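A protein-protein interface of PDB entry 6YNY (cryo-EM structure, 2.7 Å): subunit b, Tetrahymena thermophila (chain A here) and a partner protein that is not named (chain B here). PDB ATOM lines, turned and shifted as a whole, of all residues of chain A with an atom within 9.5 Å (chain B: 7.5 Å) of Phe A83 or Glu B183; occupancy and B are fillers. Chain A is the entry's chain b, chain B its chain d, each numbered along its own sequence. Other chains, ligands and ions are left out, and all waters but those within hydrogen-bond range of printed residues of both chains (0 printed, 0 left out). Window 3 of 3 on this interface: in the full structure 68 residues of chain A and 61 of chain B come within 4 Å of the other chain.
Among the printed residues, merely in contact across the chains: Val A86 with Glu B175, Ser A84 with Glu B179, Ser A84 with Glu B175, Phe A83 with Glu B179, Phe A83 with Thr B182, Val A86 with Leu B178 and Asn A82 with Glu B179.
The side-chain hydroxyl of Thr B182 is in hydrogen-bond range of the backbone carbonyl oxygen of Leu B178, at 2.9 Å.
Of the 13 printed residues of chain B, 5 touch a printed residue of chain A.
Hydrophobic or aromatic side chains of chain B within 4 Å of the printed part of chain A: Leu B178.
Of the 12 printed residues of chain A, 4 touch a printed residue of chain B.
Printed residues of chain A that touch a printed residue of chain B: Asn A82, Phe A83, Ser A84 and Val A86.
Hydrophobic or aromatic side chains of chain A within 4 Å of the printed part of chain B: Phe A83 and Val A86.
Along chain A the printed residues that touch a printed residue of chain B span positions 82 to 86.
Among the printed residues, 9 pairs touch across the chains.
Among the printed residues, no Asp or Glu carboxylate lies within 4 Å of a Lys or Arg side-chain nitrogen of the other chain.
OD1 of Asn A82 lies close to OE2 of Glu B183 (3.1 Å).
The backbone NH (N) of Phe A83 lies within hydrogen-bond range of the side-chain carboxylate (OE2) of Glu B183, 3.0 Å away.
Leu A81 touches none of the printed residues of chain B.
Phe A83 touches three residues of chain B.
Of the printed residues of chain A, Leu B178 touches Val A86.
Printed residues of chain A within 4 Å of Glu B179: Asn A82, Phe A83 and Ser A84.
Leu B181 touches none of the printed residues of chain A.
Of the printed residues of chain A, Thr B182 touches Phe A83 (3.8 Å).
Glu B183 touches just these residues of chain A: Asn A82 and Phe A83.
No residue of chain A comes within 4 Å of Thr B184.
The nearest residue of chain B that does not touch Phe A83 is Leu B178 (4.8 Å).
The nearest printed residue of chain A that does not touch Glu B175 is Lys A87 (4.2 Å).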
ATOM      1  N   ASN A  75      -3.798 -32.536  -9.143  1.00  0.00           N
ATOM      2  CA  ASN A  75      -4.024 -32.061  -7.787  1.00  0.00           C
ATOM      3  C   ASN A  75      -2.840 -32.465  -6.927  1.00  0.00           C
ATOM      4  O   ASN A  75      -2.433 -33.631  -6.932  1.00  0.00           O
ATOM      5  CB  ASN A  75      -5.317 -32.622  -7.194  1.00  0.00           C
ATOM      6  CG  ASN A  75      -5.605 -32.075  -5.819  1.00  0.00           C
ATOM      7  OD1 ASN A  75      -5.517 -30.872  -5.584  1.00  0.00           O
ATOM      8  ND2 ASN A  75      -5.937 -32.960  -4.893  1.00  0.00           N
ATOM      9  N   HIS A  78       0.670 -28.929  -2.491  1.00  0.00           N
ATOM     10  CA  HIS A  78       1.169 -27.565  -2.604  1.00  0.00           C
ATOM     11  C   HIS A  78       0.439 -26.761  -3.667  1.00  0.00           C
ATOM     12  O   HIS A  78       0.266 -25.549  -3.505  1.00  0.00           O
ATOM     13  CB  HIS A  78       2.666 -27.577  -2.917  1.00  0.00           C
ATOM     14  CG  HIS A  78       3.299 -26.224  -2.887  1.00  0.00           C
ATOM     15  ND1 HIS A  78       3.323 -25.438  -1.757  1.00  0.00           N
ATOM     16  CD2 HIS A  78       3.932 -25.516  -3.850  1.00  0.00           C
ATOM     17  CE1 HIS A  78       3.945 -24.305  -2.025  1.00  0.00           C
ATOM     18  NE2 HIS A  78       4.324 -24.327  -3.289  1.00  0.00           N
ATOM     19  N   HIS A  79       0.011 -27.405  -4.753  1.00  0.00           N
ATOM     20  CA  HIS A  79      -0.773 -26.768  -5.808  1.00  0.00           C
ATOM     21  C   HIS A  79      -2.140 -27.438  -5.873  1.00  0.00           C
ATOM     22  O   HIS A  79      -2.439 -28.175  -6.822  1.00  0.00           O
ATOM     23  CB  HIS A  79      -0.075 -26.854  -7.162  1.00  0.00           C
ATOM     24  CG  HIS A  79       1.178 -26.044  -7.257  1.00  0.00           C
ATOM     25  ND1 HIS A  79       1.174 -24.708  -7.592  1.00  0.00           N
ATOM     26  CD2 HIS A  79       2.476 -26.385  -7.084  1.00  0.00           C
ATOM     27  CE1 HIS A  79       2.415 -24.258  -7.610  1.00  0.00           C
ATOM     28  NE2 HIS A  79       3.224 -25.256  -7.304  1.00  0.00           N
ATOM     29  N   PRO A  80      -2.992 -27.209  -4.878  1.00  0.00           N
ATOM     30  CA  PRO A  80      -4.325 -27.816  -4.908  1.00  0.00           C
ATOM     31  C   PRO A  80      -5.151 -27.288  -6.068  1.00  0.00           C
ATOM     32  O   PRO A  80      -5.151 -26.092  -6.365  1.00  0.00           O
ATOM     33  CB  PRO A  80      -4.926 -27.425  -3.556  1.00  0.00           C
ATOM     34  CG  PRO A  80      -4.148 -26.259  -3.108  1.00  0.00           C
ATOM     35  CD  PRO A  80      -2.776 -26.421  -3.657  1.00  0.00           C
ATOM     36  N   LEU A  81      -5.861 -28.203  -6.724  1.00  0.00           N
ATOM     37  CA  LEU A  81      -6.630 -27.840  -7.906  1.00  0.00           C
ATOM     38  C   LEU A  81      -7.741 -26.859  -7.562  1.00  0.00           C
ATOM     39  O   LEU A  81      -7.862 -25.796  -8.181  1.00  0.00           O
ATOM     40  CB  LEU A  81      -7.203 -29.099  -8.547  1.00  0.00           C
ATOM     41  CG  LEU A  81      -8.069 -28.915  -9.788  1.00  0.00           C
ATOM     42  CD1 LEU A  81      -7.307 -28.213 -10.887  1.00  0.00           C
ATOM     43  CD2 LEU A  81      -8.560 -30.258 -10.260  1.00  0.00           C
ATOM     44  N   ASN A  82      -8.560 -27.196  -6.575  1.00  0.00           N
ATOM     45  CA  ASN A  82      -9.679 -26.360  -6.182  1.00  0.00           C
ATOM     46  C   ASN A  82      -9.255 -25.344  -5.127  1.00  0.00           C
ATOM     47  O   ASN A  82      -8.266 -25.521  -4.413  1.00  0.00           O
ATOM     48  CB  ASN A  82     -10.828 -27.219  -5.667  1.00  0.00           C
ATOM     49  CG  ASN A  82     -11.482 -28.020  -6.764  1.00  0.00           C
ATOM     50  OD1 ASN A  82     -11.850 -27.482  -7.807  1.00  0.00           O
ATOM     51  ND2 ASN A  82     -11.619 -29.314  -6.543  1.00  0.00           N
ATOM     52  N   PHE A  83     -10.033 -24.273  -5.030  1.00  0.00           N
ATOM     53  CA  PHE A  83      -9.691 -23.120  -4.217  1.00  0.00           C
ATOM     54  C   PHE A  83     -10.536 -23.057  -2.954  1.00  0.00           C
ATOM     55  O   PHE A  83     -11.703 -23.455  -2.939  1.00  0.00           O
ATOM     56  CB  PHE A  83      -9.875 -21.825  -5.006  1.00  0.00           C
ATOM     57  CG  PHE A  83      -8.966 -21.704  -6.182  1.00  0.00           C
ATOM     58  CD1 PHE A  83      -7.743 -21.083  -6.062  1.00  0.00           C
ATOM     59  CD2 PHE A  83      -9.333 -22.215  -7.406  1.00  0.00           C
ATOM     60  CE1 PHE A  83      -6.907 -20.972  -7.140  1.00  0.00           C
ATOM     61  CE2 PHE A  83      -8.499 -22.106  -8.488  1.00  0.00           C
ATOM     62  CZ  PHE A  83      -7.285 -21.485  -8.354  1.00  0.00           C
ATOM     63  N   SER A  84      -9.922 -22.539  -1.896  1.00  0.00           N
ATOM     64  CA  SER A  84     -10.594 -22.289  -0.632  1.00  0.00           C
ATOM     65  C   SER A  84      -9.763 -21.281   0.142  1.00  0.00           C
ATOM     66  O   SER A  84      -8.597 -21.038  -0.175  1.00  0.00           O
ATOM     67  CB  SER A  84     -10.774 -23.572   0.181  1.00  0.00           C
ATOM     68  OG  SER A  84      -9.520 -24.161   0.477  1.00  0.00           O
ATOM     69  N   ALA A  85     -10.383 -20.692   1.163  1.00  0.00           N
ATOM     70  CA  ALA A  85      -9.664 -19.775   2.033  1.00  0.00           C
ATOM     71  C   ALA A  85      -8.728 -20.496   2.988  1.00  0.00           C
ATOM     72  O   ALA A  85      -7.911 -19.839   3.641  1.00  0.00           O
ATOM     73  CB  ALA A  85     -10.649 -18.922   2.823  1.00  0.00           C
ATOM     74  N   VAL A  86      -8.823 -21.821   3.082  1.00  0.00           N
ATOM     75  CA  VAL A  86      -7.950 -22.569   3.976  1.00  0.00           C
ATOM     76  C   VAL A  86      -6.527 -22.582   3.441  1.00  0.00           C
ATOM     77  O   VAL A  86      -5.565 -22.387   4.193  1.00  0.00           O
ATOM     78  CB  VAL A  86      -8.490 -23.994   4.180  1.00  0.00           C
ATOM     79  CG1 VAL A  86      -7.662 -24.728   5.205  1.00  0.00           C
ATOM     80  CG2 VAL A  86      -9.937 -23.959   4.603  1.00  0.00           C
ATOM     81  N   LYS A  87      -6.365 -22.811   2.138  1.00  0.00           N
ATOM     82  CA  LYS A  87      -5.027 -22.837   1.567  1.00  0.00           C
ATOM     83  C   LYS A  87      -4.418 -21.444   1.526  1.00  0.00           C
ATOM     84  O   LYS A  87      -3.204 -21.297   1.690  1.00  0.00           O
ATOM     85  CB  LYS A  87      -5.066 -23.445   0.167  1.00  0.00           C
ATOM     86  CG  LYS A  87      -3.714 -23.588  -0.487  1.00  0.00           C
ATOM     87  CD  LYS A  87      -2.804 -24.486   0.318  1.00  0.00           C
ATOM     88  CE  LYS A  87      -1.446 -24.612  -0.316  1.00  0.00           C
ATOM     89  NZ  LYS A  87      -0.592 -25.543   0.453  1.00  0.00           N
ATOM     90  N   ILE A  88      -5.239 -20.419   1.303  1.00  0.00           N
ATOM     91  CA  ILE A  88      -4.741 -19.051   1.346  1.00  0.00           C
ATOM     92  C   ILE A  88      -4.263 -18.709   2.746  1.00  0.00           C
ATOM     93  O   ILE A  88      -3.316 -17.933   2.917  1.00  0.00           O
ATOM     94  CB  ILE A  88      -5.827 -18.072   0.867  1.00  0.00           C
ATOM     95  CG1 ILE A  88      -6.267 -18.423  -0.549  1.00  0.00           C
ATOM     96  CG2 ILE A  88      -5.311 -16.656   0.906  1.00  0.00           C
ATOM     97  CD1 ILE A  88      -7.434 -17.626  -1.036  1.00  0.00           C
ATOM     98  N   GLU B 175     -12.892 -28.381   4.914  1.00  0.00           N
ATOM     99  CA  GLU B 175     -12.217 -27.774   3.774  1.00  0.00           C
ATOM    100  C   GLU B 175     -12.795 -28.290   2.465  1.00  0.00           C
ATOM    101  O   GLU B 175     -13.022 -27.516   1.529  1.00  0.00           O
ATOM    102  CB  GLU B 175     -10.718 -28.049   3.847  1.00  0.00           C
ATOM    103  CG  GLU B 175      -9.906 -27.299   2.819  1.00  0.00           C
ATOM    104  CD  GLU B 175      -8.417 -27.500   2.987  1.00  0.00           C
ATOM    105  OE1 GLU B 175      -8.017 -28.307   3.850  1.00  0.00           O
ATOM    106  OE2 GLU B 175      -7.642 -26.846   2.258  1.00  0.00           O
ATOM    107  N   THR B 176     -13.053 -29.593   2.388  1.00  0.00           N
ATOM    108  CA  THR B 176     -13.668 -30.163   1.196  1.00  0.00           C
ATOM    109  C   THR B 176     -15.053 -29.574   0.959  1.00  0.00           C
ATOM    110  O   THR B 176     -15.396 -29.203  -0.168  1.00  0.00           O
ATOM    111  CB  THR B 176     -13.740 -31.682   1.336  1.00  0.00           C
ATOM    112  OG1 THR B 176     -12.424 -32.199   1.561  1.00  0.00           O
ATOM    113  CG2 THR B 176     -14.311 -32.311   0.095  1.00  0.00           C
ATOM    114  N   GLU B 177     -15.863 -29.476   2.012  1.00  0.00           N
ATOM    115  CA  GLU B 177     -17.176 -28.860   1.871  1.00  0.00           C
ATOM    116  C   GLU B 177     -17.052 -27.396   1.473  1.00  0.00           C
ATOM    117  O   GLU B 177     -17.824 -26.900   0.647  1.00  0.00           O
ATOM    118  CB  GLU B 177     -17.954 -28.990   3.175  1.00  0.00           C
ATOM    119  CG  GLU B 177     -18.291 -30.410   3.563  1.00  0.00           C
ATOM    120  CD  GLU B 177     -18.770 -30.524   4.994  1.00  0.00           C
ATOM    121  OE1 GLU B 177     -19.026 -29.477   5.621  1.00  0.00           O
ATOM    122  OE2 GLU B 177     -18.885 -31.661   5.495  1.00  0.00           O
ATOM    123  N   LEU B 178     -16.085 -26.689   2.056  1.00  0.00           N
ATOM    124  CA  LEU B 178     -15.883 -25.287   1.724  1.00  0.00           C
ATOM    125  C   LEU B 178     -15.421 -25.113   0.284  1.00  0.00           C
ATOM    126  O   LEU B 178     -15.725 -24.095  -0.345  1.00  0.00           O
ATOM    127  CB  LEU B 178     -14.873 -24.676   2.690  1.00  0.00           C
ATOM    128  CG  LEU B 178     -14.682 -23.166   2.651  1.00  0.00           C
ATOM    129  CD1 LEU B 178     -15.915 -22.470   3.171  1.00  0.00           C
ATOM    130  CD2 LEU B 178     -13.470 -22.785   3.466  1.00  0.00           C
ATOM    131  N   GLU B 179     -14.689 -26.089  -0.251  1.00  0.00           N
ATOM    132  CA  GLU B 179     -14.287 -26.034  -1.651  1.00  0.00           C
ATOM    133  C   GLU B 179     -15.474 -26.256  -2.577  1.00  0.00           C
ATOM    134  O   GLU B 179     -15.582 -25.609  -3.623  1.00  0.00           O
ATOM    135  CB  GLU B 179     -13.203 -27.074  -1.920  1.00  0.00           C
ATOM    136  CG  GLU B 179     -11.881 -26.789  -1.256  1.00  0.00           C
ATOM    137  CD  GLU B 179     -10.941 -27.974  -1.304  1.00  0.00           C
ATOM    138  OE1 GLU B 179     -11.186 -28.897  -2.104  1.00  0.00           O
ATOM    139  OE2 GLU B 179      -9.958 -27.984  -0.536  1.00  0.00           O
ATOM    140  N   GLU B 180     -16.372 -27.171  -2.214  1.00  0.00           N
ATOM    141  CA  GLU B 180     -17.537 -27.431  -3.050  1.00  0.00           C
ATOM    142  C   GLU B 180     -18.419 -26.195  -3.167  1.00  0.00           C
ATOM    143  O   GLU B 180     -18.947 -25.900  -4.245  1.00  0.00           O
ATOM    144  CB  GLU B 180     -18.322 -28.614  -2.486  1.00  0.00           C
ATOM    145  CG  GLU B 180     -19.570 -28.974  -3.266  1.00  0.00           C
ATOM    146  CD  GLU B 180     -20.797 -28.189  -2.840  1.00  0.00           C
ATOM    147  OE1 GLU B 180     -20.760 -27.543  -1.773  1.00  0.00           O
ATOM    148  OE2 GLU B 180     -21.803 -28.218  -3.577  1.00  0.00           O
ATOM    149  N   LEU B 181     -18.590 -25.461  -2.069  1.00  0.00           N
ATOM    150  CA  LEU B 181     -19.355 -24.222  -2.126  1.00  0.00           C
ATOM    151  C   LEU B 181     -18.687 -23.210  -3.044  1.00  0.00           C
ATOM    152  O   LEU B 181     -19.360 -22.519  -3.815  1.00  0.00           O
ATOM    153  CB  LEU B 181     -19.513 -23.641  -0.725  1.00  0.00           C
ATOM    154  CG  LEU B 181     -20.155 -24.544   0.321  1.00  0.00           C
ATOM    155  CD1 LEU B 181     -20.041 -23.912   1.686  1.00  0.00           C
ATOM    156  CD2 LEU B 181     -21.599 -24.822  -0.021  1.00  0.00           C
ATOM    157  N   THR B 182     -17.361 -23.114  -2.976  1.00  0.00           N
ATOM    158  CA  THR B 182     -16.644 -22.137  -3.784  1.00  0.00           C
ATOM    159  C   THR B 182     -16.672 -22.511  -5.260  1.00  0.00           C
ATOM    160  O   THR B 182     -16.897 -21.652  -6.118  1.00  0.00           O
ATOM    161  CB  THR B 182     -15.205 -22.017  -3.286  1.00  0.00           C
ATOM    162  OG1 THR B 182     -15.206 -21.712  -1.886  1.00  0.00           O
ATOM    163  CG2 THR B 182     -14.469 -20.934  -4.025  1.00  0.00           C
ATOM    164  N   GLU B 183     -16.454 -23.788  -5.575  1.00  0.00           N
ATOM    165  CA  GLU B 183     -16.422 -24.213  -6.968  1.00  0.00           C
ATOM    166  C   GLU B 183     -17.796 -24.179  -7.620  1.00  0.00           C
ATOM    167  O   GLU B 183     -17.880 -24.063  -8.846  1.00  0.00           O
ATOM    168  CB  GLU B 183     -15.828 -25.613  -7.072  1.00  0.00           C
ATOM    169  CG  GLU B 183     -14.397 -25.712  -6.593  1.00  0.00           C
ATOM    170  CD  GLU B 183     -13.441 -24.855  -7.398  1.00  0.00           C
ATOM    171  OE1 GLU B 183     -13.783 -24.489  -8.542  1.00  0.00           O
ATOM    172  OE2 GLU B 183     -12.350 -24.539  -6.883  1.00  0.00           O
ATOM    173  N   THR B 184     -18.868 -24.283  -6.842  1.00  0.00           N
ATOM    174  CA  THR B 184     -20.219 -24.136  -7.362  1.00  0.00           C
ATOM    175  C   THR B 184     -20.750 -22.718  -7.219  1.00  0.00           C
ATOM    176  O   THR B 184     -21.913 -22.470  -7.545  1.00  0.00           O
ATOM    177  CB  THR B 184     -21.167 -25.110  -6.662  1.00  0.00           C
ATOM    178  OG1 THR B 184     -21.078 -24.947  -5.243  1.00  0.00           O
ATOM    179  CG2 THR B 184     -20.818 -26.527  -7.027  1.00  0.00           C
ATOM    180  N   HIS B 185     -19.921 -21.789  -6.753  1.00  0.00           N
ATOM    181  CA  HIS B 185     -20.308 -20.391  -6.589  1.00  0.00           C
ATOM    182  C   HIS B 185     -21.523 -20.250  -5.678  1.00  0.00           C
ATOM    183  O   HIS B 185     -22.408 -19.426  -5.910  1.00  0.00           O
ATOM    184  CB  HIS B 185     -20.549 -19.729  -7.943  1.00  0.00           C
ATOM    185  CG  HIS B 185     -19.301 -19.236  -8.599  1.00  0.00           C
ATOM    186  ND1 HIS B 185     -19.310 -18.285  -9.594  1.00  0.00           N
ATOM    187  CD2 HIS B 185     -18.002 -19.557  -8.397  1.00  0.00           C
ATOM    188  CE1 HIS B 185     -18.071 -18.043  -9.979  1.00  0.00           C
ATOM    189  NE2 HIS B 185     -17.258 -18.802  -9.270  1.00  0.00           N
ATOM    190  N   ASN B 186     -21.561 -21.062  -4.627  1.00  0.00           N
ATOM    191  CA  ASN B 186     -22.523 -20.886  -3.544  1.00  0.00           C
ATOM    192  C   ASN B 186     -21.895 -20.041  -2.438  1.00  0.00           C
ATOM    193  O   ASN B 186     -21.764 -20.449  -1.285  1.00  0.00           O
ATOM    194  CB  ASN B 186     -22.992 -22.238  -3.022  1.00  0.00           C
ATOM    195  CG  ASN B 186     -24.064 -22.855  -3.885  1.00  0.00           C
ATOM    196  OD1 ASN B 186     -25.245 -22.546  -3.744  1.00  0.00           O
ATOM    197  ND2 ASN B 186     -23.662 -23.738  -4.783  1.00  0.00           N
ATOM    198  N   HIS B 217     -28.872 -20.041  -4.747  1.00  0.00           N
ATOM    199  CA  HIS B 217     -27.671 -19.744  -5.509  1.00  0.00           C
ATOM    200  C   HIS B 217     -27.666 -18.285  -5.949  1.00  0.00           C
ATOM    201  O   HIS B 217     -28.711 -17.749  -6.326  1.00  0.00           O
ATOM    202  CB  HIS B 217     -27.578 -20.646  -6.738  1.00  0.00           C
ATOM    203  CG  HIS B 217     -26.213 -20.703  -7.344  1.00  0.00           C
ATOM    204  ND1 HIS B 217     -25.765 -19.779  -8.260  1.00  0.00           N
ATOM    205  CD2 HIS B 217     -25.198 -21.578  -7.163  1.00  0.00           C
ATOM    206  CE1 HIS B 217     -24.528 -20.079  -8.614  1.00  0.00           C
ATOM    207  NE2 HIS B 217     -24.162 -21.169  -7.967  1.00  0.00           N
